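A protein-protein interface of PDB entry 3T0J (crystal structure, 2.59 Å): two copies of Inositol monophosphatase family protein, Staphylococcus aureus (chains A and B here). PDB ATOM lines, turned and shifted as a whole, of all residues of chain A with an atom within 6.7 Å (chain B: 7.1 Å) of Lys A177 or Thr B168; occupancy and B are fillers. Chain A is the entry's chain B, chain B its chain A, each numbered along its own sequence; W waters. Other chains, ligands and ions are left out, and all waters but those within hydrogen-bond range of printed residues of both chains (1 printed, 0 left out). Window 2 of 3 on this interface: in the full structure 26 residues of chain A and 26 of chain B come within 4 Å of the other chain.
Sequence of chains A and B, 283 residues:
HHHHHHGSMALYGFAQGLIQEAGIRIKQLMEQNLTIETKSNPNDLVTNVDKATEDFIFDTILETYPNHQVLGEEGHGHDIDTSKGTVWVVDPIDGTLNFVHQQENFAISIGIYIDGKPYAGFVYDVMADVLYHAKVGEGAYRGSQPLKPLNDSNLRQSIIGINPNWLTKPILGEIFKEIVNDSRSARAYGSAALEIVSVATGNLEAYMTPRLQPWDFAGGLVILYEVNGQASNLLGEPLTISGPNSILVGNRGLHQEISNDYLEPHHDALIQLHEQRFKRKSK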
ATOM      1  N   LEU A 167     -34.164  28.528 -19.053  1.00  0.00           N
ATOM      2  CA  LEU A 167     -33.163  29.287 -19.749  1.00  0.00           C
ATOM      3  C   LEU A 167     -33.690  29.890 -21.043  1.00  0.00           C
ATOM      4  O   LEU A 167     -33.105  30.833 -21.553  1.00  0.00           O
ATOM      5  CB  LEU A 167     -31.924  28.427 -19.972  1.00  0.00           C
ATOM      6  CG  LEU A 167     -30.872  28.509 -18.847  1.00  0.00           C
ATOM      7  CD1 LEU A 167     -31.476  29.039 -17.555  1.00  0.00           C
ATOM      8  CD2 LEU A 167     -30.174  27.193 -18.585  1.00  0.00           C
ATOM      9  N   LEU A 172     -35.559  35.612 -17.762  1.00  0.00           N
ATOM     10  CA  LEU A 172     -35.218  34.498 -16.903  1.00  0.00           C
ATOM     11  C   LEU A 172     -33.902  33.882 -17.306  1.00  0.00           C
ATOM     12  O   LEU A 172     -33.032  33.648 -16.475  1.00  0.00           O
ATOM     13  CB  LEU A 172     -36.328  33.460 -16.944  1.00  0.00           C
ATOM     14  CG  LEU A 172     -36.785  33.036 -15.548  1.00  0.00           C
ATOM     15  CD1 LEU A 172     -36.402  34.065 -14.441  1.00  0.00           C
ATOM     16  CD2 LEU A 172     -38.290  32.748 -15.535  1.00  0.00           C
ATOM     17  N   GLY A 173     -33.781  33.628 -18.600  1.00  0.00           N
ATOM     18  CA  GLY A 173     -32.559  33.156 -19.191  1.00  0.00           C
ATOM     19  C   GLY A 173     -31.382  33.990 -18.752  1.00  0.00           C
ATOM     20  O   GLY A 173     -30.373  33.428 -18.362  1.00  0.00           O
ATOM     21  N   GLU A 174     -31.484  35.317 -18.798  1.00  0.00           N
ATOM     22  CA  GLU A 174     -30.310  36.121 -18.476  1.00  0.00           C
ATOM     23  C   GLU A 174     -29.941  36.026 -16.983  1.00  0.00           C
ATOM     24  O   GLU A 174     -28.750  35.917 -16.625  1.00  0.00           O
ATOM     25  CB  GLU A 174     -30.460  37.577 -18.949  1.00  0.00           C
ATOM     26  CG  GLU A 174     -29.180  38.441 -18.768  1.00  0.00           C
ATOM     27  CD  GLU A 174     -27.934  37.901 -19.524  1.00  0.00           C
ATOM     28  OE1 GLU A 174     -28.085  37.257 -20.608  1.00  0.00           O
ATOM     29  OE2 GLU A 174     -26.802  38.133 -19.020  1.00  0.00           O
ATOM     30  N   ILE A 175     -30.950  36.024 -16.116  1.00  0.00           N
ATOM     31  CA  ILE A 175     -30.684  35.900 -14.691  1.00  0.00           C
ATOM     32  C   ILE A 175     -30.110  34.553 -14.221  1.00  0.00           C
ATOM     33  O   ILE A 175     -29.567  34.516 -13.143  1.00  0.00           O
ATOM     34  CB  ILE A 175     -31.898  36.301 -13.794  1.00  0.00           C
ATOM     35  CG1 ILE A 175     -32.912  35.164 -13.668  1.00  0.00           C
ATOM     36  CG2 ILE A 175     -32.549  37.604 -14.257  1.00  0.00           C
ATOM     37  CD1 ILE A 175     -32.888  34.509 -12.283  1.00  0.00           C
ATOM     38  N   PHE A 176     -30.218  33.469 -14.990  1.00  0.00           N
ATOM     39  CA  PHE A 176     -29.684  32.170 -14.547  1.00  0.00           C
ATOM     40  C   PHE A 176     -28.435  31.784 -15.343  1.00  0.00           C
ATOM     41  O   PHE A 176     -27.769  30.801 -15.025  1.00  0.00           O
ATOM     42  CB  PHE A 176     -30.675  31.023 -14.761  1.00  0.00           C
ATOM     43  CG  PHE A 176     -31.822  30.955 -13.786  1.00  0.00           C
ATOM     44  CD1 PHE A 176     -31.614  30.937 -12.425  1.00  0.00           C
ATOM     45  CD2 PHE A 176     -33.116  30.797 -14.259  1.00  0.00           C
ATOM     46  CE1 PHE A 176     -32.689  30.820 -11.536  1.00  0.00           C
ATOM     47  CE2 PHE A 176     -34.208  30.686 -13.387  1.00  0.00           C
ATOM     48  CZ  PHE A 176     -33.984  30.692 -12.020  1.00  0.00           C
ATOM     49  N   LYS A 177     -28.164  32.523 -16.412  1.00  0.00           N
ATOM     50  CA  LYS A 177     -27.050  32.258 -17.315  1.00  0.00           C
ATOM     51  C   LYS A 177     -25.746  32.059 -16.539  1.00  0.00           C
ATOM     52  O   LYS A 177     -25.049  31.072 -16.746  1.00  0.00           O
ATOM     53  CB  LYS A 177     -26.891  33.454 -18.268  1.00  0.00           C
ATOM     54  CG  LYS A 177     -26.244  33.151 -19.594  1.00  0.00           C
ATOM     55  CD  LYS A 177     -25.605  34.402 -20.173  1.00  0.00           C
ATOM     56  CE  LYS A 177     -25.034  34.180 -21.612  1.00  0.00           C
ATOM     57  NZ  LYS A 177     -24.142  32.970 -21.767  1.00  0.00           N
ATOM     58  N   GLU A 178     -25.428  32.996 -15.648  1.00  0.00           N
ATOM     59  CA  GLU A 178     -24.177  32.963 -14.918  1.00  0.00           C
ATOM     60  C   GLU A 178     -24.114  31.750 -14.071  1.00  0.00           C
ATOM     61  O   GLU A 178     -23.101  31.020 -14.029  1.00  0.00           O
ATOM     62  CB  GLU A 178     -24.075  34.147 -13.961  1.00  0.00           C
ATOM     63  CG  GLU A 178     -23.135  35.212 -14.376  1.00  0.00           C
ATOM     64  CD  GLU A 178     -23.498  35.705 -15.691  1.00  0.00           C
ATOM     65  OE1 GLU A 178     -23.498  34.881 -16.628  1.00  0.00           O
ATOM     66  OE2 GLU A 178     -23.791  36.907 -15.777  1.00  0.00           O
ATOM     67  N   ILE A 179     -25.195  31.540 -13.355  1.00  0.00           N
ATOM     68  CA  ILE A 179     -25.170  30.451 -12.445  1.00  0.00           C
ATOM     69  C   ILE A 179     -24.972  29.094 -13.158  1.00  0.00           C
ATOM     70  O   ILE A 179     -24.191  28.285 -12.681  1.00  0.00           O
ATOM     71  CB  ILE A 179     -26.229  30.628 -11.307  1.00  0.00           C
ATOM     72  CG1 ILE A 179     -26.397  29.416 -10.390  1.00  0.00           C
ATOM     73  CG2 ILE A 179     -27.463  31.252 -11.785  1.00  0.00           C
ATOM     74  CD1 ILE A 179     -26.727  28.111 -11.066  1.00  0.00           C
ATOM     75  N   VAL A 180     -25.558  28.881 -14.336  1.00  0.00           N
ATOM     76  CA  VAL A 180     -25.220  27.641 -15.041  1.00  0.00           C
ATOM     77  C   VAL A 180     -23.828  27.616 -15.700  1.00  0.00           C
ATOM     78  O   VAL A 180     -23.196  26.567 -15.741  1.00  0.00           O
ATOM     79  CB  VAL A 180     -26.372  27.009 -15.947  1.00  0.00           C
ATOM     80  CG1 VAL A 180     -27.665  27.756 -15.858  1.00  0.00           C
ATOM     81  CG2 VAL A 180     -25.914  26.728 -17.388  1.00  0.00           C
ATOM     82  N   ASN A 181     -23.336  28.758 -16.167  1.00  0.00           N
ATOM     83  CA  ASN A 181     -21.987  28.811 -16.759  1.00  0.00           C
ATOM     84  C   ASN A 181     -20.884  28.515 -15.757  1.00  0.00           C
ATOM     85  O   ASN A 181     -19.833  27.962 -16.061  1.00  0.00           O
ATOM     86  CB  ASN A 181     -21.717  30.180 -17.383  1.00  0.00           C
ATOM     87  CG  ASN A 181     -22.301  30.306 -18.771  1.00  0.00           C
ATOM     88  OD1 ASN A 181     -22.397  29.318 -19.508  1.00  0.00           O
ATOM     89  ND2 ASN A 181     -22.686  31.539 -19.153  1.00  0.00           N
ATOM     90  N   ASP A 182     -21.154  28.899 -14.544  1.00  0.00           N
ATOM     91  CA  ASP A 182     -20.195  28.872 -13.497  1.00  0.00           C
ATOM     92  C   ASP A 182     -20.087  27.581 -12.682  1.00  0.00           C
ATOM     93  O   ASP A 182     -18.983  27.214 -12.248  1.00  0.00           O
ATOM     94  CB  ASP A 182     -20.629  29.937 -12.561  1.00  0.00           C
ATOM     95  CG  ASP A 182     -19.531  30.649 -12.063  1.00  0.00           C
ATOM     96  OD1 ASP A 182     -18.909  31.367 -12.905  1.00  0.00           O
ATOM     97  OD2 ASP A 182     -19.279  30.431 -10.853  1.00  0.00           O
ATOM     98  N   ASN B 163     -28.441  18.799 -21.462  1.00  0.00           N
ATOM     99  CA  ASN B 163     -27.872  19.527 -20.318  1.00  0.00           C
ATOM    100  C   ASN B 163     -28.073  21.024 -20.465  1.00  0.00           C
ATOM    101  O   ASN B 163     -27.742  21.599 -21.505  1.00  0.00           O
ATOM    102  CB  ASN B 163     -26.410  19.224 -20.136  1.00  0.00           C
ATOM    103  CG  ASN B 163     -25.857  19.733 -18.800  1.00  0.00           C
ATOM    104  OD1 ASN B 163     -25.287  18.965 -18.032  1.00  0.00           O
ATOM    105  ND2 ASN B 163     -25.989  21.017 -18.534  1.00  0.00           N
ATOM    106  N   PRO B 164     -28.640  21.665 -19.437  1.00  0.00           N
ATOM    107  CA  PRO B 164     -28.764  23.113 -19.373  1.00  0.00           C
ATOM    108  C   PRO B 164     -27.532  23.909 -19.786  1.00  0.00           C
ATOM    109  O   PRO B 164     -27.671  25.015 -20.275  1.00  0.00           O
ATOM    110  CB  PRO B 164     -29.062  23.374 -17.884  1.00  0.00           C
ATOM    111  CG  PRO B 164     -29.624  22.050 -17.349  1.00  0.00           C
ATOM    112  CD  PRO B 164     -29.479  21.009 -18.428  1.00  0.00           C
ATOM    113  N   ASN B 165     -26.340  23.387 -19.586  1.00  0.00           N
ATOM    114  CA  ASN B 165     -25.137  24.106 -19.996  1.00  0.00           C
ATOM    115  C   ASN B 165     -25.032  24.459 -21.458  1.00  0.00           C
ATOM    116  O   ASN B 165     -24.513  25.507 -21.787  1.00  0.00           O
ATOM    117  CB  ASN B 165     -23.916  23.321 -19.612  1.00  0.00           C
ATOM    118  CG  ASN B 165     -23.524  23.579 -18.225  1.00  0.00           C
ATOM    119  OD1 ASN B 165     -23.062  24.680 -17.920  1.00  0.00           O
ATOM    120  ND2 ASN B 165     -23.727  22.589 -17.332  1.00  0.00           N
ATOM    121  N   TRP B 166     -25.527  23.586 -22.332  1.00  0.00           N
ATOM    122  CA  TRP B 166     -25.493  23.828 -23.758  1.00  0.00           C
ATOM    123  C   TRP B 166     -26.356  25.003 -24.149  1.00  0.00           C
ATOM    124  O   TRP B 166     -26.084  25.650 -25.164  1.00  0.00           O
ATOM    125  CB  TRP B 166     -25.943  22.592 -24.527  1.00  0.00           C
ATOM    126  CG  TRP B 166     -25.120  21.415 -24.213  1.00  0.00           C
ATOM    127  CD1 TRP B 166     -25.567  20.196 -23.869  1.00  0.00           C
ATOM    128  CD2 TRP B 166     -23.682  21.356 -24.153  1.00  0.00           C
ATOM    129  NE1 TRP B 166     -24.517  19.362 -23.600  1.00  0.00           N
ATOM    130  CE2 TRP B 166     -23.343  20.041 -23.769  1.00  0.00           C
ATOM    131  CE3 TRP B 166     -22.645  22.288 -24.403  1.00  0.00           C
ATOM    132  CZ2 TRP B 166     -22.016  19.602 -23.656  1.00  0.00           C
ATOM    133  CZ3 TRP B 166     -21.316  21.867 -24.281  1.00  0.00           C
ATOM    134  CH2 TRP B 166     -21.015  20.522 -23.903  1.00  0.00           C
ATOM    135  N   LEU B 167     -27.389  25.297 -23.359  1.00  0.00           N
ATOM    136  CA  LEU B 167     -28.275  26.391 -23.725  1.00  0.00           C
ATOM    137  C   LEU B 167     -27.659  27.793 -23.565  1.00  0.00           C
ATOM    138  O   LEU B 167     -28.230  28.786 -24.005  1.00  0.00           O
ATOM    139  CB  LEU B 167     -29.638  26.254 -23.026  1.00  0.00           C
ATOM    140  CG  LEU B 167     -30.709  25.581 -23.906  1.00  0.00           C
ATOM    141  CD1 LEU B 167     -30.352  24.130 -24.130  1.00  0.00           C
ATOM    142  CD2 LEU B 167     -32.084  25.697 -23.240  1.00  0.00           C
ATOM    143  N   THR B 168     -26.482  27.847 -22.957  1.00  0.00           N
ATOM    144  CA  THR B 168     -25.777  29.089 -22.717  1.00  0.00           C
ATOM    145  C   THR B 168     -24.569  29.307 -23.646  1.00  0.00           C
ATOM    146  O   THR B 168     -23.888  30.338 -23.530  1.00  0.00           O
ATOM    147  CB  THR B 168     -25.243  29.123 -21.296  1.00  0.00           C
ATOM    148  OG1 THR B 168     -24.146  28.207 -21.169  1.00  0.00           O
ATOM    149  CG2 THR B 168     -26.335  28.762 -20.323  1.00  0.00           C
ATOM    150  N   LYS B 169     -24.285  28.350 -24.537  1.00  0.00           N
ATOM    151  CA  LYS B 169     -23.128  28.496 -25.441  1.00  0.00           C
ATOM    152  C   LYS B 169     -23.410  29.436 -26.641  1.00  0.00           C
ATOM    153  O   LYS B 169     -24.458  29.328 -27.288  1.00  0.00           O
ATOM    154  CB  LYS B 169     -22.596  27.128 -25.931  1.00  0.00           C
ATOM    155  CG  LYS B 169     -22.300  26.119 -24.854  1.00  0.00           C
ATOM    156  CD  LYS B 169     -21.082  26.499 -24.054  1.00  0.00           C
ATOM    157  CE  LYS B 169     -21.275  26.207 -22.564  1.00  0.00           C
ATOM    158  NZ  LYS B 169     -20.069  25.554 -22.030  1.00  0.00           N
ATOM    159  N   PRO B 170     -22.480  30.363 -26.937  1.00  0.00           N
ATOM    160  CA  PRO B 170     -22.621  31.231 -28.096  1.00  0.00           C
ATOM    161  C   PRO B 170     -23.078  30.454 -29.352  1.00  0.00           C
ATOM    162  O   PRO B 170     -22.407  29.481 -29.753  1.00  0.00           O
ATOM    163  CB  PRO B 170     -21.200  31.782 -28.291  1.00  0.00           C
ATOM    164  CG  PRO B 170     -20.493  31.582 -27.015  1.00  0.00           C
ATOM    165  CD  PRO B 170     -21.362  30.781 -26.083  1.00  0.00           C
ATOM    166  N   ILE B 171     -24.222  30.868 -29.919  1.00  0.00           N
ATOM    167  CA  ILE B 171     -24.821  30.345 -31.177  1.00  0.00           C
ATOM    168  C   ILE B 171     -25.568  29.010 -31.028  1.00  0.00           C
ATOM    169  O   ILE B 171     -26.730  28.863 -31.455  1.00  0.00           O
ATOM    170  CB  ILE B 171     -23.814  30.373 -32.410  1.00  0.00           C
ATOM    171  CG1 ILE B 171     -23.658  31.802 -32.947  1.00  0.00           C
ATOM    172  CG2 ILE B 171     -24.230  29.395 -33.538  1.00  0.00           C
ATOM    173  CD1 ILE B 171     -24.994  32.690 -32.990  1.00  0.00           C
ATOM    174  N   LEU B 172     -24.893  28.043 -30.414  1.00  0.00           N
ATOM    175  CA  LEU B 172     -25.508  26.766 -30.055  1.00  0.00           C
ATOM    176  C   LEU B 172     -26.705  26.979 -29.125  1.00  0.00           C
ATOM    177  O   LEU B 172     -27.784  26.454 -29.385  1.00  0.00           O
ATOM    178  CB  LEU B 172     -24.462  25.871 -29.418  1.00  0.00           C
ATOM    179  CG  LEU B 172     -24.814  24.430 -29.079  1.00  0.00           C
ATOM    180  CD1 LEU B 172     -25.011  23.551 -30.328  1.00  0.00           C
ATOM    181  CD2 LEU B 172     -23.681  23.914 -28.162  1.00  0.00           C
ATOM    182  N   GLY B 173     -26.526  27.777 -28.071  1.00  0.00           N
ATOM    183  CA  GLY B 173     -27.631  28.210 -27.207  1.00  0.00           C
ATOM    184  C   GLY B 173     -28.914  28.603 -27.954  1.00  0.00           C
ATOM    185  O   GLY B 173     -29.992  28.063 -27.685  1.00  0.00           O
ATOM    186  N   GLU B 174     -28.792  29.529 -28.909  1.00  0.00           N
ATOM    187  CA  GLU B 174     -29.954  30.026 -29.655  1.00  0.00           C
ATOM    188  C   GLU B 174     -30.664  28.932 -30.441  1.00  0.00           C
ATOM    189  O   GLU B 174     -31.893  28.878 -30.442  1.00  0.00           O
ATOM    190  CB  GLU B 174     -29.588  31.223 -30.551  1.00  0.00           C
ATOM    191  CG  GLU B 174     -29.453  32.557 -29.792  1.00  0.00           C
ATOM    192  CD  GLU B 174     -30.686  32.890 -28.907  1.00  0.00           C
ATOM    193  OE1 GLU B 174     -30.490  33.341 -27.743  1.00  0.00           O
ATOM    194  OE2 GLU B 174     -31.848  32.688 -29.368  1.00  0.00           O
ATOM    195  N   LYS B 177     -32.365  26.540 -27.756  1.00  0.00           N
ATOM    196  CA  LYS B 177     -33.479  27.249 -27.145  1.00  0.00           C
ATOM    197  C   LYS B 177     -34.763  27.049 -27.936  1.00  0.00           C
ATOM    198  O   LYS B 177     -35.808  26.808 -27.356  1.00  0.00           O
ATOM    199  CB  LYS B 177     -33.178  28.747 -27.020  1.00  0.00           C
ATOM    200  CG  LYS B 177     -32.837  29.239 -25.581  1.00  0.00           C
ATOM    201  CD  LYS B 177     -31.331  29.336 -25.275  1.00  0.00           C
ATOM    202  CE  LYS B 177     -31.013  30.567 -24.397  1.00  0.00           C
ATOM    203  NZ  LYS B 177     -31.206  31.867 -25.123  1.00  0.00           N
HETATM  204  O   HOH W   1     -23.136  24.048 -14.818  1.00  0.00           O
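Water W1 bridges the backbone carbonyl oxygen of Val A180 and the side-chain amide nitrogen of Asn B165.
Of the 12 printed residues of chain A, 4 touch a printed residue of chain B.
Along chain A the printed residues that touch a printed residue of chain B span positions 167 to 181.
Leu A167 touches Lys B177, but with the chains exchanged Lys A177 does not touch Leu B167 (6.3 Å).
Positions printed for both chains: 167, 172, 173, 174 and 177.
Lys A177 touches just one residue of chain B: Thr B168 (3.2 Å).
Thr B168 touches just these residues of chain A: Lys A177, Val A180 and Asn A181.
Of the printed residues of chain B, Asn A181 touches Thr B168.
Printed residues of chain A within 4 Å of Lys B177: Leu A167 (3.5 Å).
Of the printed residues of chain A, Asn B165 touches Val A180 (2.9 Å).
Of the printed residues of chain A, Pro B164 touches Leu A167 (3.7 Å) and Val A180 (3.8 Å).
Printed residues of chain B within 4 Å of Leu A167: Pro B164 (3.7 Å) and Lys B177 (3.5 Å).
Phe A176 touches none of the printed residues of chain B.
The nearest printed residue of chain A that does not touch Asn B165 is Asn A181 (4.4 Å).
The side-chain amide oxygen (OD1) of Asn B165 sits close to the backbone carbonyl oxygen (O) of Val A180 (2.9 Å).
The side-chain amino group (NZ) of Lys A177 sits at hydrogen-bond distance from the backbone carbonyl oxygen (O) of Thr B168, 3.2 Å away.
The side-chain hydroxyl (OG1) of Thr B168 is in hydrogen-bond range of the side-chain amide oxygen (OD1) of Asn A181, 2.7 Å away.
Among the printed residues, pairs that only touch across the chains: Leu A167 with Pro B164 (3.7 Å), Leu A167 with Lys B177 (3.5 Å), Val A180 with Pro B164 (3.8 Å) and Val A180 with Thr B168 (3.6 Å).
N of Asn B165 lies close to ND2 of Asn B163.
The side-chain hydroxyl of Thr B168 lies within hydrogen-bond range of the backbone carbonyl oxygen of Asn B165, at 2.8 Å.
The side-chain carboxylate (OE1) of Glu B174 lies within salt-bridge range of the side-chain amino group (NZ) of Lys B177 (3.1 Å).
The side-chain amino group (NZ) of Lys A177 sits close to the side-chain amide nitrogen (ND2) of Asn A181, at 3.3 Å.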
